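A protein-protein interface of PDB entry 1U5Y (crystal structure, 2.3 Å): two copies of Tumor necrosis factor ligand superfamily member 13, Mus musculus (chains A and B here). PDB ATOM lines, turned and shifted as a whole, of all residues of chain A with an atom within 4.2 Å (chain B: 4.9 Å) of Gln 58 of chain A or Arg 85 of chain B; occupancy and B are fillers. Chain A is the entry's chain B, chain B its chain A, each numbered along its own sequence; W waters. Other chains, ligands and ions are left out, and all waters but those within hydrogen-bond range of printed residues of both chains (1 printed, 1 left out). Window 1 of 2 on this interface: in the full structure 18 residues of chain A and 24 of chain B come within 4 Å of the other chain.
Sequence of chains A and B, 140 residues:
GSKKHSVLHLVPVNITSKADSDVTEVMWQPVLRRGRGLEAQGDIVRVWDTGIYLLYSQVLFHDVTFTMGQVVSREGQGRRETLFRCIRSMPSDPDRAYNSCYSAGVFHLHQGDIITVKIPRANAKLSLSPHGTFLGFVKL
The backbone carbonyl oxygen (O) of Arg 85 of chain B sits at hydrogen-bond distance from the side-chain amide nitrogen (NE2) of Gln 58 of chain A (2.9 Å).
The backbone carbonyl oxygen of His 131 of chain A is in hydrogen-bond range of the backbone NH of Arg 85 of chain B (3.0 Å).
The side-chain sulfur (SG) of Cys 86 of chain B sits close to the side-chain hydroxyl (OG) of Ser 100 of chain A (3.7 Å).
The side-chain hydroxyl of Ser 100 of chain A is in hydrogen-bond range of the backbone NH of Ile 87 of chain B (2.8 Å).
The side-chain hydroxyl of Ser 103 of chain B is in hydrogen-bond range of the side-chain amide oxygen of Gln 58 of chain A (2.7 Å).
The backbone NH (N) of Cys 86 of chain B sits at hydrogen-bond distance from the backbone carbonyl oxygen (O) of Gln 70 of chain B, at 3.0 Å.
The backbone NH (N) of Tyr 102 of chain B lies within hydrogen-bond range of the side-chain sulfur (SG) of Cys 86 of chain B (3.5 Å).
The backbone carbonyl oxygen (O) of Gly 132 of chain A lies within hydrogen-bond range of the side-chain amide nitrogen (NE2) of Gln 58 of chain A (3.0 Å).
The backbone carbonyl oxygen (O) of Gln 58 of chain A lies within hydrogen-bond range of the backbone NH (N) of Phe 134 of chain A (3.0 Å).
Among the printed residues, merely in contact across the chains: Tyr 102 of chain A with Tyr 102 of chain B (3.5 Å), His 131 of chain A with Leu 83 of chain B (3.9 Å), His 131 of chain A with Phe 84 of chain B (3.4 Å), Phe 134 of chain A with Phe 84 of chain B (3.7 Å) and Phe 134 of chain A with Ser 103 of chain B (3.6 Å).
Of chain B, only Arg 85 and Ser 103 come within 4 Å of Gln 58 of chain A.
Cys 101 of chain A touches none of the printed residues of chain B.
Printed residues of chain B within 4 Å of His 131 of chain A: Leu 83, Phe 84 and Arg 85.
Thr 133 of chain A touches none of the printed residues of chain B.
Of chain A, only Gln 58 (2.9 Å) and His 131 (3.0 Å) come within 4 Å of Arg 85 of chain B.
Of the printed residues of chain A, Tyr 102 of chain B touches Tyr 102 (3.5 Å).
The nearest printed residue of chain A that does not touch Arg 85 of chain B is Ser 100 of chain A (4.4 Å).
The nearest printed residue of chain A that does not touch Cys 86 of chain B is Gln 58 of chain A (4.8 Å).
Printed residues of chain B that touch a printed residue of chain A: Leu 83, Phe 84, Arg 85, Cys 86, Ile 87, Tyr 102 and Ser 103.
Hydrophobic or aromatic side chains of chain A within 4 Å of the printed part of chain B: Tyr 102 and Phe 134.
Among the printed residues, no Asp or Glu carboxylate lies within 4 Å of a Lys or Arg side-chain nitrogen of the other chain.
Tyr 102 of chain B touches its own counterpart, Tyr 102 of chain A.
2 positions are printed for both chains.
Water W1 lies within hydrogen-bond range of OH of Tyr 102 of chain A and OH of Tyr 102 of chain B.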
ATOM      1  N   SER A  57       3.927  20.369 -21.175  1.00  0.00           N
ATOM      2  CA  SER A  57       4.744  21.397 -20.552  1.00  0.00           C
ATOM      3  C   SER A  57       4.596  22.744 -21.258  1.00  0.00           C
ATOM      4  O   SER A  57       4.712  22.838 -22.481  1.00  0.00           O
ATOM      5  CB  SER A  57       6.202  20.956 -20.579  1.00  0.00           C
ATOM      6  OG  SER A  57       7.053  22.000 -20.176  1.00  0.00           O
ATOM      7  N   GLN A  58       4.309  23.781 -20.486  1.00  0.00           N
ATOM      8  CA  GLN A  58       4.359  25.143 -20.996  1.00  0.00           C
ATOM      9  C   GLN A  58       5.210  26.019 -20.080  1.00  0.00           C
ATOM     10  O   GLN A  58       5.184  25.870 -18.856  1.00  0.00           O
ATOM     11  CB  GLN A  58       2.963  25.712 -21.152  1.00  0.00           C
ATOM     12  CG  GLN A  58       2.923  27.152 -21.712  1.00  0.00           C
ATOM     13  CD  GLN A  58       1.506  27.656 -21.978  1.00  0.00           C
ATOM     14  OE1 GLN A  58       0.794  27.100 -22.818  1.00  0.00           O
ATOM     15  NE2 GLN A  58       1.101  28.717 -21.269  1.00  0.00           N
ATOM     16  N   VAL A  59       6.009  26.896 -20.680  1.00  0.00           N
ATOM     17  CA  VAL A  59       6.767  27.889 -19.925  1.00  0.00           C
ATOM     18  C   VAL A  59       6.552  29.260 -20.578  1.00  0.00           C
ATOM     19  O   VAL A  59       6.733  29.442 -21.781  1.00  0.00           O
ATOM     20  CB  VAL A  59       8.266  27.566 -19.872  1.00  0.00           C
ATOM     21  CG1 VAL A  59       9.027  28.685 -19.157  1.00  0.00           C
ATOM     22  CG2 VAL A  59       8.518  26.212 -19.173  1.00  0.00           C
ATOM     23  N   GLN A  70      12.199  25.045 -23.225  1.00  0.00           N
ATOM     24  CA  GLN A  70      12.450  24.094 -22.146  1.00  0.00           C
ATOM     25  C   GLN A  70      12.705  22.679 -22.663  1.00  0.00           C
ATOM     26  O   GLN A  70      12.380  22.367 -23.807  1.00  0.00           O
ATOM     27  CB  GLN A  70      11.325  24.137 -21.090  1.00  0.00           C
ATOM     28  CG  GLN A  70      10.008  23.444 -21.452  1.00  0.00           C
ATOM     29  CD  GLN A  70       9.089  24.301 -22.284  1.00  0.00           C
ATOM     30  OE1 GLN A  70       9.514  25.309 -22.862  1.00  0.00           O
ATOM     31  NE2 GLN A  70       7.810  23.922 -22.329  1.00  0.00           N
ATOM     32  N   SER A 100       4.620  32.035 -24.763  1.00  0.00           N
ATOM     33  CA  SER A 100       4.458  30.791 -24.054  1.00  0.00           C
ATOM     34  C   SER A 100       4.926  29.694 -24.991  1.00  0.00           C
ATOM     35  O   SER A 100       4.663  29.728 -26.200  1.00  0.00           O
ATOM     36  CB  SER A 100       3.016  30.588 -23.625  1.00  0.00           C
ATOM     37  OG  SER A 100       2.134  30.804 -24.696  1.00  0.00           O
ATOM     38  N   CYS A 101       5.637  28.732 -24.416  1.00  0.00           N
ATOM     39  CA  CYS A 101       6.256  27.661 -25.152  1.00  0.00           C
ATOM     40  C   CYS A 101       5.618  26.383 -24.650  1.00  0.00           C
ATOM     41  O   CYS A 101       5.822  26.010 -23.485  1.00  0.00           O
ATOM     42  CB  CYS A 101       7.774  27.670 -24.917  1.00  0.00           C
ATOM     43  SG  CYS A 101       8.726  27.218 -26.374  1.00  0.00           S
ATOM     44  N   TYR A 102       4.817  25.751 -25.519  1.00  0.00           N
ATOM     45  CA  TYR A 102       4.065  24.528 -25.198  1.00  0.00           C
ATOM     46  C   TYR A 102       4.540  23.316 -26.005  1.00  0.00           C
ATOM     47  O   TYR A 102       4.735  23.383 -27.215  1.00  0.00           O
ATOM     48  CB  TYR A 102       2.574  24.692 -25.448  1.00  0.00           C
ATOM     49  CG  TYR A 102       1.749  23.490 -24.974  1.00  0.00           C
ATOM     50  CD1 TYR A 102       1.153  23.466 -23.714  1.00  0.00           C
ATOM     51  CD2 TYR A 102       1.574  22.384 -25.792  1.00  0.00           C
ATOM     52  CE1 TYR A 102       0.400  22.362 -23.281  1.00  0.00           C
ATOM     53  CE2 TYR A 102       0.846  21.290 -25.374  1.00  0.00           C
ATOM     54  CZ  TYR A 102       0.251  21.288 -24.121  1.00  0.00           C
ATOM     55  OH  TYR A 102      -0.474  20.189 -23.769  1.00  0.00           O
ATOM     56  N   HIS A 131      -1.087  29.947 -14.617  1.00  0.00           N
ATOM     57  CA  HIS A 131      -1.776  29.963 -15.914  1.00  0.00           C
ATOM     58  C   HIS A 131      -0.817  30.013 -17.112  1.00  0.00           C
ATOM     59  O   HIS A 131      -1.226  29.739 -18.239  1.00  0.00           O
ATOM     60  CB  HIS A 131      -2.724  31.176 -16.043  1.00  0.00           C
ATOM     61  CG  HIS A 131      -3.382  31.585 -14.762  1.00  0.00           C
ATOM     62  ND1 HIS A 131      -3.206  32.833 -14.201  1.00  0.00           N
ATOM     63  CD2 HIS A 131      -4.237  30.921 -13.946  1.00  0.00           C
ATOM     64  CE1 HIS A 131      -3.905  32.909 -13.080  1.00  0.00           C
ATOM     65  NE2 HIS A 131      -4.545  31.766 -12.906  1.00  0.00           N
ATOM     66  N   GLY A 132       0.429  30.413 -16.888  1.00  0.00           N
ATOM     67  CA  GLY A 132       1.383  30.599 -17.978  1.00  0.00           C
ATOM     68  C   GLY A 132       2.476  29.551 -18.011  1.00  0.00           C
ATOM     69  O   GLY A 132       3.036  29.241 -19.054  1.00  0.00           O
ATOM     70  N   THR A 133       2.800  29.023 -16.848  1.00  0.00           N
ATOM     71  CA  THR A 133       3.840  28.023 -16.706  1.00  0.00           C
ATOM     72  C   THR A 133       3.273  26.832 -15.938  1.00  0.00           C
ATOM     73  O   THR A 133       2.766  26.976 -14.840  1.00  0.00           O
ATOM     74  CB  THR A 133       5.023  28.642 -15.972  1.00  0.00           C
ATOM     75  OG1 THR A 133       5.508  29.759 -16.736  1.00  0.00           O
ATOM     76  CG2 THR A 133       6.195  27.687 -15.906  1.00  0.00           C
ATOM     77  N   PHE A 134       3.331  25.662 -16.539  1.00  0.00           N
ATOM     78  CA  PHE A 134       2.790  24.474 -15.901  1.00  0.00           C
ATOM     79  C   PHE A 134       3.313  23.183 -16.512  1.00  0.00           C
ATOM     80  O   PHE A 134       3.921  23.186 -17.593  1.00  0.00           O
ATOM     81  CB  PHE A 134       1.250  24.493 -15.908  1.00  0.00           C
ATOM     82  CG  PHE A 134       0.638  24.735 -17.246  1.00  0.00           C
ATOM     83  CD1 PHE A 134       0.153  25.995 -17.582  1.00  0.00           C
ATOM     84  CD2 PHE A 134       0.528  23.716 -18.173  1.00  0.00           C
ATOM     85  CE1 PHE A 134      -0.413  26.223 -18.812  1.00  0.00           C
ATOM     86  CE2 PHE A 134      -0.045  23.949 -19.403  1.00  0.00           C
ATOM     87  CZ  PHE A 134      -0.534  25.202 -19.710  1.00  0.00           C
ATOM     88  N   GLN B  70      -4.924  33.958 -26.159  1.00  0.00           N
ATOM     89  CA  GLN B  70      -6.256  33.701 -25.660  1.00  0.00           C
ATOM     90  C   GLN B  70      -6.138  33.278 -24.211  1.00  0.00           C
ATOM     91  O   GLN B  70      -5.064  32.819 -23.786  1.00  0.00           O
ATOM     92  CB  GLN B  70      -6.932  32.619 -26.502  1.00  0.00           C
ATOM     93  CG  GLN B  70      -6.402  31.225 -26.338  1.00  0.00           C
ATOM     94  CD  GLN B  70      -5.250  30.917 -27.251  1.00  0.00           C
ATOM     95  OE1 GLN B  70      -4.587  31.831 -27.764  1.00  0.00           O
ATOM     96  NE2 GLN B  70      -5.009  29.624 -27.473  1.00  0.00           N
ATOM     97  N   VAL B  71      -7.235  33.457 -23.468  1.00  0.00           N
ATOM     98  CA  VAL B  71      -7.363  33.080 -22.056  1.00  0.00           C
ATOM     99  C   VAL B  71      -8.526  32.093 -21.895  1.00  0.00           C
ATOM    100  O   VAL B  71      -9.656  32.376 -22.282  1.00  0.00           O
ATOM    101  CB  VAL B  71      -7.673  34.309 -21.167  1.00  0.00           C
ATOM    102  CG1 VAL B  71      -7.682  33.922 -19.664  1.00  0.00           C
ATOM    103  CG2 VAL B  71      -6.674  35.422 -21.430  1.00  0.00           C
ATOM    104  N   LEU B  83      -7.684  29.112 -16.149  1.00  0.00           N
ATOM    105  CA  LEU B  83      -7.100  27.781 -16.219  1.00  0.00           C
ATOM    106  C   LEU B  83      -5.740  27.870 -16.896  1.00  0.00           C
ATOM    107  O   LEU B  83      -4.737  27.396 -16.351  1.00  0.00           O
ATOM    108  CB  LEU B  83      -8.003  26.830 -17.033  1.00  0.00           C
ATOM    109  CG  LEU B  83      -9.462  26.784 -16.605  1.00  0.00           C
ATOM    110  CD1 LEU B  83     -10.176  25.674 -17.369  1.00  0.00           C
ATOM    111  CD2 LEU B  83      -9.529  26.573 -15.071  1.00  0.00           C
ATOM    112  N   PHE B  84      -5.717  28.477 -18.086  1.00  0.00           N
ATOM    113  CA  PHE B  84      -4.466  28.718 -18.776  1.00  0.00           C
ATOM    114  C   PHE B  84      -4.572  29.766 -19.843  1.00  0.00           C
ATOM    115  O   PHE B  84      -5.651  30.127 -20.285  1.00  0.00           O
ATOM    116  CB  PHE B  84      -3.913  27.428 -19.393  1.00  0.00           C
ATOM    117  CG  PHE B  84      -4.775  26.831 -20.473  1.00  0.00           C
ATOM    118  CD1 PHE B  84      -4.566  27.150 -21.799  1.00  0.00           C
ATOM    119  CD2 PHE B  84      -5.760  25.906 -20.163  1.00  0.00           C
ATOM    120  CE1 PHE B  84      -5.358  26.583 -22.800  1.00  0.00           C
ATOM    121  CE2 PHE B  84      -6.550  25.327 -21.159  1.00  0.00           C
ATOM    122  CZ  PHE B  84      -6.352  25.655 -22.468  1.00  0.00           C
ATOM    123  N   ARG B  85      -3.412  30.242 -20.259  1.00  0.00           N
ATOM    124  CA  ARG B  85      -3.317  31.313 -21.228  1.00  0.00           C
ATOM    125  C   ARG B  85      -2.175  31.030 -22.199  1.00  0.00           C
ATOM    126  O   ARG B  85      -1.129  30.496 -21.820  1.00  0.00           O
ATOM    127  CB  ARG B  85      -3.151  32.656 -20.495  1.00  0.00           C
ATOM    128  CG  ARG B  85      -1.964  33.481 -20.894  1.00  0.00           C
ATOM    129  CD  ARG B  85      -2.080  34.968 -20.608  1.00  0.00           C
ATOM    130  NE  ARG B  85      -3.016  35.310 -19.541  1.00  0.00           N
ATOM    131  CZ  ARG B  85      -3.726  36.435 -19.516  1.00  0.00           C
ATOM    132  NH1 ARG B  85      -3.619  37.327 -20.502  1.00  0.00           N
ATOM    133  NH2 ARG B  85      -4.556  36.675 -18.501  1.00  0.00           N
ATOM    134  N   CYS B  86      -2.399  31.378 -23.457  1.00  0.00           N
ATOM    135  CA  CYS B  86      -1.387  31.243 -24.477  1.00  0.00           C
ATOM    136  C   CYS B  86      -0.958  32.654 -24.835  1.00  0.00           C
ATOM    137  O   CYS B  86      -1.794  33.527 -25.057  1.00  0.00           O
ATOM    138  CB  CYS B  86      -1.972  30.526 -25.681  1.00  0.00           C
ATOM    139  SG  CYS B  86      -0.748  30.045 -26.899  1.00  0.00           S
ATOM    140  N   ILE B  87       0.338  32.899 -24.872  1.00  0.00           N
ATOM    141  CA  ILE B  87       0.848  34.200 -25.274  1.00  0.00           C
ATOM    142  C   ILE B  87       1.795  34.042 -26.459  1.00  0.00           C
ATOM    143  O   ILE B  87       2.702  33.188 -26.461  1.00  0.00           O
ATOM    144  CB  ILE B  87       1.572  34.892 -24.105  1.00  0.00           C
ATOM    145  CG1 ILE B  87       0.570  35.190 -22.983  1.00  0.00           C
ATOM    146  CG2 ILE B  87       2.205  36.183 -24.568  1.00  0.00           C
ATOM    147  CD1 ILE B  87       1.183  35.471 -21.632  1.00  0.00           C
ATOM    148  N   TYR B 102      -1.269  27.627 -29.354  1.00  0.00           N
ATOM    149  CA  TYR B 102      -1.858  26.398 -28.834  1.00  0.00           C
ATOM    150  C   TYR B 102      -1.450  26.293 -27.381  1.00  0.00           C
ATOM    151  O   TYR B 102      -0.291  26.455 -27.058  1.00  0.00           O
ATOM    152  CB  TYR B 102      -1.343  25.167 -29.604  1.00  0.00           C
ATOM    153  CG  TYR B 102      -1.903  23.860 -29.090  1.00  0.00           C
ATOM    154  CD1 TYR B 102      -3.017  23.261 -29.683  1.00  0.00           C
ATOM    155  CD2 TYR B 102      -1.352  23.248 -27.974  1.00  0.00           C
ATOM    156  CE1 TYR B 102      -3.551  22.074 -29.173  1.00  0.00           C
ATOM    157  CE2 TYR B 102      -1.861  22.053 -27.479  1.00  0.00           C
ATOM    158  CZ  TYR B 102      -2.964  21.475 -28.079  1.00  0.00           C
ATOM    159  OH  TYR B 102      -3.433  20.296 -27.571  1.00  0.00           O
ATOM    160  N   SER B 103      -2.417  26.072 -26.511  1.00  0.00           N
ATOM    161  CA  SER B 103      -2.145  25.610 -25.159  1.00  0.00           C
ATOM    162  C   SER B 103      -3.205  24.594 -24.726  1.00  0.00           C
ATOM    163  O   SER B 103      -4.272  24.453 -25.324  1.00  0.00           O
ATOM    164  CB  SER B 103      -2.058  26.779 -24.179  1.00  0.00           C
ATOM    165  OG  SER B 103      -1.746  26.344 -22.854  1.00  0.00           O
ATOM    166  N   PRO B 120      -7.994  39.073 -25.197  1.00  0.00           N
ATOM    167  CA  PRO B 120      -8.208  40.353 -24.526  1.00  0.00           C
ATOM    168  C   PRO B 120      -7.812  41.582 -25.373  1.00  0.00           C
ATOM    169  O   PRO B 120      -7.157  42.470 -24.846  1.00  0.00           O
ATOM    170  CB  PRO B 120      -7.345  40.227 -23.248  1.00  0.00           C
ATOM    171  CG  PRO B 120      -6.206  39.342 -23.656  1.00  0.00           C
ATOM    172  CD  PRO B 120      -6.707  38.468 -24.790  1.00  0.00           C
HETATM  173  O   HOH W   1      -1.557  18.882 -26.014  1.00  0.00           O
